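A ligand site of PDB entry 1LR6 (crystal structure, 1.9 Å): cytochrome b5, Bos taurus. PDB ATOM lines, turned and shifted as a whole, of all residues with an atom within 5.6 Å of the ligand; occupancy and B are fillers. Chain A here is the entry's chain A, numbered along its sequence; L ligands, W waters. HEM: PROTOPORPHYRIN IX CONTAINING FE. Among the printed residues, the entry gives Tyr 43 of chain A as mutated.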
ATOM      1  N   LEU A  21      25.302   8.348  36.611  1.00  0.00           N
ATOM      2  CA  LEU A  21      26.100   9.546  36.777  1.00  0.00           C
ATOM      3  C   LEU A  21      25.234  10.574  37.453  1.00  0.00           C
ATOM      4  O   LEU A  21      24.006  10.413  37.518  1.00  0.00           O
ATOM      5  CB  LEU A  21      26.669  10.046  35.443  1.00  0.00           C
ATOM      6  CG  LEU A  21      25.844  10.362  34.217  1.00  0.00           C
ATOM      7  CD1 LEU A  21      24.926  11.546  34.468  1.00  0.00           C
ATOM      8  CD2 LEU A  21      26.813  10.683  33.066  1.00  0.00           C
ATOM      9  N   LEU A  23      24.078  14.661  37.868  1.00  0.00           N
ATOM     10  CA  LEU A  23      23.958  15.962  37.232  1.00  0.00           C
ATOM     11  C   LEU A  23      23.102  16.799  38.170  1.00  0.00           C
ATOM     12  O   LEU A  23      21.944  16.449  38.430  1.00  0.00           O
ATOM     13  CB  LEU A  23      23.259  15.871  35.865  1.00  0.00           C
ATOM     14  CG  LEU A  23      23.883  15.033  34.742  1.00  0.00           C
ATOM     15  CD1 LEU A  23      22.917  14.956  33.552  1.00  0.00           C
ATOM     16  CD2 LEU A  23      25.204  15.644  34.331  1.00  0.00           C
ATOM     17  N   TYR A  28      21.167   9.758  37.496  1.00  0.00           N
ATOM     18  CA  TYR A  28      20.627   9.279  36.221  1.00  0.00           C
ATOM     19  C   TYR A  28      21.151   7.912  35.842  1.00  0.00           C
ATOM     20  O   TYR A  28      22.350   7.675  35.929  1.00  0.00           O
ATOM     21  CB  TYR A  28      20.985  10.245  35.082  1.00  0.00           C
ATOM     22  CG  TYR A  28      20.474  11.656  35.258  1.00  0.00           C
ATOM     23  CD1 TYR A  28      21.034  12.493  36.220  1.00  0.00           C
ATOM     24  CD2 TYR A  28      19.420  12.133  34.481  1.00  0.00           C
ATOM     25  CE1 TYR A  28      20.548  13.786  36.411  1.00  0.00           C
ATOM     26  CE2 TYR A  28      18.923  13.435  34.668  1.00  0.00           C
ATOM     27  CZ  TYR A  28      19.491  14.250  35.636  1.00  0.00           C
ATOM     28  OH  TYR A  28      19.019  15.522  35.847  1.00  0.00           O
ATOM     29  N   LEU A  30      21.806   5.902  32.832  1.00  0.00           N
ATOM     30  CA  LEU A  30      21.904   6.047  31.389  1.00  0.00           C
ATOM     31  C   LEU A  30      22.285   4.750  30.679  1.00  0.00           C
ATOM     32  O   LEU A  30      22.681   4.763  29.521  1.00  0.00           O
ATOM     33  CB  LEU A  30      22.930   7.124  31.048  1.00  0.00           C
ATOM     34  CG  LEU A  30      22.605   8.477  31.675  1.00  0.00           C
ATOM     35  CD1 LEU A  30      23.626   9.527  31.206  1.00  0.00           C
ATOM     36  CD2 LEU A  30      21.194   8.886  31.277  1.00  0.00           C
ATOM     37  N   PHE A  33      20.661   4.426  27.431  1.00  0.00           N
ATOM     38  CA  PHE A  33      20.783   5.627  26.605  1.00  0.00           C
ATOM     39  C   PHE A  33      22.133   5.756  25.894  1.00  0.00           C
ATOM     40  O   PHE A  33      22.241   6.440  24.868  1.00  0.00           O
ATOM     41  CB  PHE A  33      20.533   6.857  27.481  1.00  0.00           C
ATOM     42  CG  PHE A  33      20.588   8.161  26.730  1.00  0.00           C
ATOM     43  CD1 PHE A  33      21.584   9.092  27.012  1.00  0.00           C
ATOM     44  CD2 PHE A  33      19.634   8.453  25.764  1.00  0.00           C
ATOM     45  CE1 PHE A  33      21.627  10.308  26.336  1.00  0.00           C
ATOM     46  CE2 PHE A  33      19.671   9.669  25.075  1.00  0.00           C
ATOM     47  CZ  PHE A  33      20.673  10.601  25.370  1.00  0.00           C
ATOM     48  N   HIS A  37      22.798   8.301  22.621  1.00  0.00           N
ATOM     49  CA  HIS A  37      23.370   9.617  22.843  1.00  0.00           C
ATOM     50  C   HIS A  37      24.051  10.225  21.612  1.00  0.00           C
ATOM     51  O   HIS A  37      25.032   9.685  21.102  1.00  0.00           O
ATOM     52  CB  HIS A  37      24.366   9.558  23.993  1.00  0.00           C
ATOM     53  CG  HIS A  37      25.004  10.874  24.318  1.00  0.00           C
ATOM     54  ND1 HIS A  37      26.359  11.075  24.404  1.00  0.00           N
ATOM     55  CD2 HIS A  37      24.431  12.062  24.627  1.00  0.00           C
ATOM     56  CE1 HIS A  37      26.579  12.347  24.761  1.00  0.00           C
ATOM     57  NE2 HIS A  37      25.436  12.991  24.905  1.00  0.00           N
ATOM     58  N   PRO A  38      23.543  11.375  21.137  1.00  0.00           N
ATOM     59  CA  PRO A  38      24.118  12.034  19.971  1.00  0.00           C
ATOM     60  C   PRO A  38      25.622  12.270  20.105  1.00  0.00           C
ATOM     61  O   PRO A  38      26.379  12.058  19.166  1.00  0.00           O
ATOM     62  CB  PRO A  38      23.333  13.344  19.889  1.00  0.00           C
ATOM     63  CG  PRO A  38      21.986  12.934  20.392  1.00  0.00           C
ATOM     64  CD  PRO A  38      22.336  12.082  21.598  1.00  0.00           C
ATOM     65  N   GLY A  39      26.047  12.681  21.298  1.00  0.00           N
ATOM     66  CA  GLY A  39      27.462  12.939  21.522  1.00  0.00           C
ATOM     67  C   GLY A  39      28.352  11.715  21.573  1.00  0.00           C
ATOM     68  O   GLY A  39      29.572  11.841  21.640  1.00  0.00           O
ATOM     69  N   TYR A  43      31.973   9.805  25.988  1.00  0.00           N
ATOM     70  CA  TYR A  43      31.844  10.911  26.932  1.00  0.00           C
ATOM     71  C   TYR A  43      31.044  10.516  28.155  1.00  0.00           C
ATOM     72  O   TYR A  43      31.284  11.028  29.249  1.00  0.00           O
ATOM     73  CB  TYR A  43      31.193  12.114  26.243  1.00  0.00           C
ATOM     74  CG  TYR A  43      31.989  12.665  25.083  1.00  0.00           C
ATOM     75  CD1 TYR A  43      33.310  13.090  25.256  1.00  0.00           C
ATOM     76  CD2 TYR A  43      31.430  12.764  23.816  1.00  0.00           C
ATOM     77  CE1 TYR A  43      34.046  13.593  24.189  1.00  0.00           C
ATOM     78  CE2 TYR A  43      32.160  13.266  22.737  1.00  0.00           C
ATOM     79  CZ  TYR A  43      33.468  13.676  22.939  1.00  0.00           C
ATOM     80  OH  TYR A  43      34.194  14.181  21.877  1.00  0.00           O
ATOM     81  N   LEU A  44      30.076   9.620  27.974  1.00  0.00           N
ATOM     82  CA  LEU A  44      29.236   9.169  29.081  1.00  0.00           C
ATOM     83  C   LEU A  44      29.935   8.143  29.972  1.00  0.00           C
ATOM     84  O   LEU A  44      29.883   8.246  31.201  1.00  0.00           O
ATOM     85  CB  LEU A  44      27.927   8.581  28.547  1.00  0.00           C
ATOM     86  CG  LEU A  44      26.992   9.543  27.788  1.00  0.00           C
ATOM     87  CD1 LEU A  44      25.736   8.818  27.353  1.00  0.00           C
ATOM     88  CD2 LEU A  44      26.638  10.700  28.694  1.00  0.00           C
ATOM     89  N   GLN A  47      32.529   9.445  32.348  1.00  0.00           N
ATOM     90  CA  GLN A  47      32.007  10.151  33.524  1.00  0.00           C
ATOM     91  C   GLN A  47      31.180   9.262  34.450  1.00  0.00           C
ATOM     92  O   GLN A  47      30.812   9.677  35.548  1.00  0.00           O
ATOM     93  CB  GLN A  47      31.151  11.333  33.074  1.00  0.00           C
ATOM     94  CG  GLN A  47      31.933  12.417  32.359  1.00  0.00           C
ATOM     95  CD  GLN A  47      33.035  12.978  33.234  1.00  0.00           C
ATOM     96  OE1 GLN A  47      32.788  13.516  34.314  1.00  0.00           O
ATOM     97  NE2 GLN A  47      34.276  12.854  32.773  1.00  0.00           N
ATOM     98  N   ALA A  52      28.960  14.532  36.767  1.00  0.00           N
ATOM     99  CA  ALA A  52      29.323  15.056  35.459  1.00  0.00           C
ATOM    100  C   ALA A  52      28.641  16.386  35.159  1.00  0.00           C
ATOM    101  O   ALA A  52      28.542  16.792  34.002  1.00  0.00           O
ATOM    102  CB  ALA A  52      28.948  14.048  34.394  1.00  0.00           C
ATOM    103  N   ASN A  55      30.880  19.020  33.172  1.00  0.00           N
ATOM    104  CA  ASN A  55      31.128  18.606  31.786  1.00  0.00           C
ATOM    105  C   ASN A  55      29.868  18.781  30.949  1.00  0.00           C
ATOM    106  O   ASN A  55      29.918  19.230  29.808  1.00  0.00           O
ATOM    107  CB  ASN A  55      31.574  17.152  31.720  1.00  0.00           C
ATOM    108  CG  ASN A  55      32.759  16.866  32.600  1.00  0.00           C
ATOM    109  OD1 ASN A  55      32.645  16.861  33.820  1.00  0.00           O
ATOM    110  ND2 ASN A  55      33.913  16.643  31.985  1.00  0.00           N
ATOM    111  N   PHE A  56      28.737  18.416  31.548  1.00  0.00           N
ATOM    112  CA  PHE A  56      27.424  18.510  30.920  1.00  0.00           C
ATOM    113  C   PHE A  56      27.112  19.946  30.518  1.00  0.00           C
ATOM    114  O   PHE A  56      26.665  20.211  29.403  1.00  0.00           O
ATOM    115  CB  PHE A  56      26.361  18.019  31.912  1.00  0.00           C
ATOM    116  CG  PHE A  56      24.957  18.027  31.379  1.00  0.00           C
ATOM    117  CD1 PHE A  56      24.541  17.077  30.450  1.00  0.00           C
ATOM    118  CD2 PHE A  56      24.039  18.973  31.815  1.00  0.00           C
ATOM    119  CE1 PHE A  56      23.233  17.058  29.978  1.00  0.00           C
ATOM    120  CE2 PHE A  56      22.726  18.964  31.352  1.00  0.00           C
ATOM    121  CZ  PHE A  56      22.320  18.006  30.427  1.00  0.00           C
ATOM    122  N   VAL A  59      29.611  21.572  27.692  1.00  0.00           N
ATOM    123  CA  VAL A  59      29.313  21.303  26.298  1.00  0.00           C
ATOM    124  C   VAL A  59      28.114  22.142  25.852  1.00  0.00           C
ATOM    125  O   VAL A  59      28.006  22.512  24.695  1.00  0.00           O
ATOM    126  CB  VAL A  59      28.989  19.816  26.076  1.00  0.00           C
ATOM    127  CG1 VAL A  59      30.236  18.972  26.269  1.00  0.00           C
ATOM    128  CG2 VAL A  59      27.929  19.378  27.046  1.00  0.00           C
ATOM    129  N   GLY A  60      27.230  22.449  26.806  1.00  0.00           N
ATOM    130  CA  GLY A  60      26.067  23.270  26.509  1.00  0.00           C
ATOM    131  C   GLY A  60      24.899  22.546  25.857  1.00  0.00           C
ATOM    132  O   GLY A  60      24.651  22.708  24.664  1.00  0.00           O
ATOM    133  N   HIS A  61      24.170  21.756  26.645  1.00  0.00           N
ATOM    134  CA  HIS A  61      23.027  21.005  26.124  1.00  0.00           C
ATOM    135  C   HIS A  61      21.792  21.854  25.879  1.00  0.00           C
ATOM    136  O   HIS A  61      21.516  22.803  26.607  1.00  0.00           O
ATOM    137  CB  HIS A  61      22.672  19.852  27.054  1.00  0.00           C
ATOM    138  CG  HIS A  61      23.634  18.713  26.989  1.00  0.00           C
ATOM    139  ND1 HIS A  61      24.884  18.710  27.574  1.00  0.00           N
ATOM    140  CD2 HIS A  61      23.544  17.541  26.302  1.00  0.00           C
ATOM    141  CE1 HIS A  61      25.490  17.565  27.215  1.00  0.00           C
ATOM    142  NE2 HIS A  61      24.715  16.838  26.445  1.00  0.00           N
ATOM    143  N   SER A  62      21.042  21.477  24.840  1.00  0.00           N
ATOM    144  CA  SER A  62      19.829  22.167  24.446  1.00  0.00           C
ATOM    145  C   SER A  62      18.721  21.925  25.456  1.00  0.00           C
ATOM    146  O   SER A  62      18.827  21.040  26.307  1.00  0.00           O
ATOM    147  CB  SER A  62      19.355  21.669  23.073  1.00  0.00           C
ATOM    148  OG  SER A  62      18.927  20.312  23.141  1.00  0.00           O
ATOM    149  N   ASP A  64      15.911  20.744  24.783  1.00  0.00           N
ATOM    150  CA  ASP A  64      15.324  19.457  24.456  1.00  0.00           C
ATOM    151  C   ASP A  64      16.063  18.304  25.141  1.00  0.00           C
ATOM    152  O   ASP A  64      15.441  17.389  25.670  1.00  0.00           O
ATOM    153  CB  ASP A  64      15.308  19.232  22.943  1.00  0.00           C
ATOM    154  CG  ASP A  64      14.346  20.153  22.223  1.00  0.00           C
ATOM    155  OD1 ASP A  64      13.149  20.198  22.595  1.00  0.00           O
ATOM    156  OD2 ASP A  64      14.770  20.834  21.268  1.00  0.00           O
ATOM    157  N   ALA A  65      17.394  18.354  25.119  1.00  0.00           N
ATOM    158  CA  ALA A  65      18.188  17.306  25.746  1.00  0.00           C
ATOM    159  C   ALA A  65      17.904  17.278  27.237  1.00  0.00           C
ATOM    160  O   ALA A  65      17.753  16.212  27.837  1.00  0.00           O
ATOM    161  CB  ALA A  65      19.671  17.555  25.500  1.00  0.00           C
ATOM    162  N   LEU A  68      14.692  15.701  27.946  1.00  0.00           N
ATOM    163  CA  LEU A  68      14.815  14.258  27.765  1.00  0.00           C
ATOM    164  C   LEU A  68      15.520  13.581  28.930  1.00  0.00           C
ATOM    165  O   LEU A  68      15.119  12.499  29.363  1.00  0.00           O
ATOM    166  CB  LEU A  68      15.572  13.965  26.470  1.00  0.00           C
ATOM    167  CG  LEU A  68      15.827  12.472  26.205  1.00  0.00           C
ATOM    168  CD1 LEU A  68      14.501  11.742  26.110  1.00  0.00           C
ATOM    169  CD2 LEU A  68      16.635  12.307  24.938  1.00  0.00           C
ATOM    170  N   SER A  69      16.582  14.218  29.428  1.00  0.00           N
ATOM    171  CA  SER A  69      17.356  13.652  30.538  1.00  0.00           C
ATOM    172  C   SER A  69      16.483  13.310  31.742  1.00  0.00           C
ATOM    173  O   SER A  69      16.769  12.355  32.482  1.00  0.00           O
ATOM    174  CB  SER A  69      18.459  14.633  30.970  1.00  0.00           C
ATOM    175  OG  SER A  69      17.921  15.766  31.632  1.00  0.00           O
ATOM    176  N   PHE A  72      15.345   9.735  32.717  1.00  0.00           N
ATOM    177  CA  PHE A  72      16.350   8.808  33.225  1.00  0.00           C
ATOM    178  C   PHE A  72      16.722   8.969  34.697  1.00  0.00           C
ATOM    179  O   PHE A  72      17.629   8.296  35.200  1.00  0.00           O
ATOM    180  CB  PHE A  72      17.615   8.926  32.366  1.00  0.00           C
ATOM    181  CG  PHE A  72      17.392   8.646  30.894  1.00  0.00           C
ATOM    182  CD1 PHE A  72      16.946   7.405  30.455  1.00  0.00           C
ATOM    183  CD2 PHE A  72      17.609   9.653  29.952  1.00  0.00           C
ATOM    184  CE1 PHE A  72      16.730   7.156  29.086  1.00  0.00           C
ATOM    185  CE2 PHE A  72      17.392   9.421  28.598  1.00  0.00           C
ATOM    186  CZ  PHE A  72      16.947   8.174  28.166  1.00  0.00           C
HETATM  187  CHA HEM L   1      25.169  16.125  22.526  1.00  0.00           C
HETATM  188  CHB HEM L   1      21.581  14.438  25.323  1.00  0.00           C
HETATM  189  CHC HEM L   1      24.775  13.860  28.908  1.00  0.00           C
HETATM  190  CHD HEM L   1      28.405  15.214  26.023  1.00  0.00           C
HETATM  191  C1A HEM L   1      23.896  15.796  23.028  1.00  0.00           C
HETATM  192  C2A HEM L   1      22.663  16.022  22.307  1.00  0.00           C
HETATM  193  C3A HEM L   1      21.677  15.502  23.074  1.00  0.00           C
HETATM  194  C4A HEM L   1      22.285  15.025  24.294  1.00  0.00           C
HETATM  195  CMA HEM L   1      20.204  15.409  22.697  1.00  0.00           C
HETATM  196  CAA HEM L   1      22.423  16.735  20.989  1.00  0.00           C
HETATM  197  CBA HEM L   1      22.660  18.238  21.046  1.00  0.00           C
HETATM  198  CGA HEM L   1      21.799  18.906  22.095  1.00  0.00           C
HETATM  199  O1A HEM L   1      20.563  18.767  22.021  1.00  0.00           O
HETATM  200  O2A HEM L   1      22.368  19.578  22.983  1.00  0.00           O
HETATM  201  C1B HEM L   1      22.167  14.091  26.525  1.00  0.00           C
HETATM  202  C2B HEM L   1      21.423  13.602  27.671  1.00  0.00           C
HETATM  203  C3B HEM L   1      22.300  13.510  28.714  1.00  0.00           C
HETATM  204  C4B HEM L   1      23.601  13.909  28.185  1.00  0.00           C
HETATM  205  CMB HEM L   1      19.937  13.248  27.673  1.00  0.00           C
HETATM  206  CAB HEM L   1      22.031  13.231  30.059  1.00  0.00           C
HETATM  207  CBB HEM L   1      21.055  12.381  30.551  1.00  0.00           C
HETATM  208  C1C HEM L   1      26.039  14.181  28.441  1.00  0.00           C
HETATM  209  C2C HEM L   1      27.215  14.192  29.266  1.00  0.00           C
HETATM  210  C3C HEM L   1      28.260  14.576  28.478  1.00  0.00           C
HETATM  211  C4C HEM L   1      27.684  14.805  27.151  1.00  0.00           C
HETATM  212  CMC HEM L   1      27.211  13.861  30.771  1.00  0.00           C
HETATM  213  CAC HEM L   1      29.617  14.800  28.793  1.00  0.00           C
HETATM  214  CBC HEM L   1      30.328  14.462  29.947  1.00  0.00           C
HETATM  215  C1D HEM L   1      27.819  15.549  24.799  1.00  0.00           C
HETATM  216  C2D HEM L   1      28.547  15.960  23.605  1.00  0.00           C
HETATM  217  C3D HEM L   1      27.642  16.240  22.658  1.00  0.00           C
HETATM  218  C4D HEM L   1      26.345  16.002  23.240  1.00  0.00           C
HETATM  219  CMD HEM L   1      30.044  16.054  23.399  1.00  0.00           C
HETATM  220  CAD HEM L   1      27.971  16.729  21.236  1.00  0.00           C
HETATM  221  CBD HEM L   1      28.045  18.247  21.184  1.00  0.00           C
HETATM  222  CGD HEM L   1      28.616  18.772  19.870  1.00  0.00           C
HETATM  223  O1D HEM L   1      28.680  20.013  19.709  1.00  0.00           O
HETATM  224  O2D HEM L   1      29.001  17.951  19.012  1.00  0.00           O
HETATM  225  NA  HEM L   1      23.661  15.227  24.270  1.00  0.00           N
HETATM  226  NB  HEM L   1      23.515  14.281  26.840  1.00  0.00           N
HETATM  227  NC  HEM L   1      26.321  14.598  27.155  1.00  0.00           N
HETATM  228  ND  HEM L   1      26.458  15.555  24.557  1.00  0.00           N
HETATM  229 FE   HEM L   1      24.986  14.913  25.687  1.00  0.00          FE
HETATM  230  O   HOH W   1      19.322  18.349  19.505  1.00  0.00           O
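Merely in contact with the ligand: Asn 55 (3.5 Å), Ser 69 (3.5 Å), Gly 39 (3.5 Å), Leu 44 (3.5 Å), Gln 47 (3.5 Å), Phe 33 (3.6 Å), Tyr 43 (3.6 Å), Ala 65 (3.6 Å), Leu 30 (3.6 Å), Phe 56 (3.6 Å), Pro 38 (3.7 Å), Leu 21 (3.9 Å) and Leu 23 (3.995 Å). Hydrophobic or aromatic side chains that line the ligand: Leu 21, Leu 23, Leu 30, Phe 33, His 37, Pro 38, Tyr 43, Leu 44, Phe 56, His 61 and Ala 65. Within 4 Å of the ligand: Leu 21, Leu 23, Leu 30, Phe 33, His 37, Pro 38, Gly 39, Tyr 43, Leu 44, Gln 47, Asn 55, Phe 56, His 61, Ser 62, Ala 65 and Ser 69.
An iron atom (FE) of the ligand is bound by a ring nitrogen (NE2) of His 61 (2.1 Å). A ring nitrogen (NE2) of His 37 binds an iron atom (FE) of the ligand. O2A of the ligand sits at hydrogen-bond distance from N of Ser 62. An oxygen (O1A) of the ligand lies within hydrogen-bond range of the side-chain hydroxyl of Ser 62, at 2.5 Å.
ND1 of His 61 sits at hydrogen-bond distance from O of Phe 56 (3.0 Å). The side-chain hydroxyl (OG) of Ser 62 is in hydrogen-bond range of the backbone NH (N) of Ala 65, 3.2 Å away. The backbone NH of Asp 64 lies close to the side-chain hydroxyl of Ser 62 (3.5 Å). The side-chain amide oxygen (OD1) of Asn 55 lies close to the side-chain amide oxygen (OE1) of Gln 47, 3.4 Å away. N of Tyr 28 is in hydrogen-bond range of O of Leu 21 (2.9 Å).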
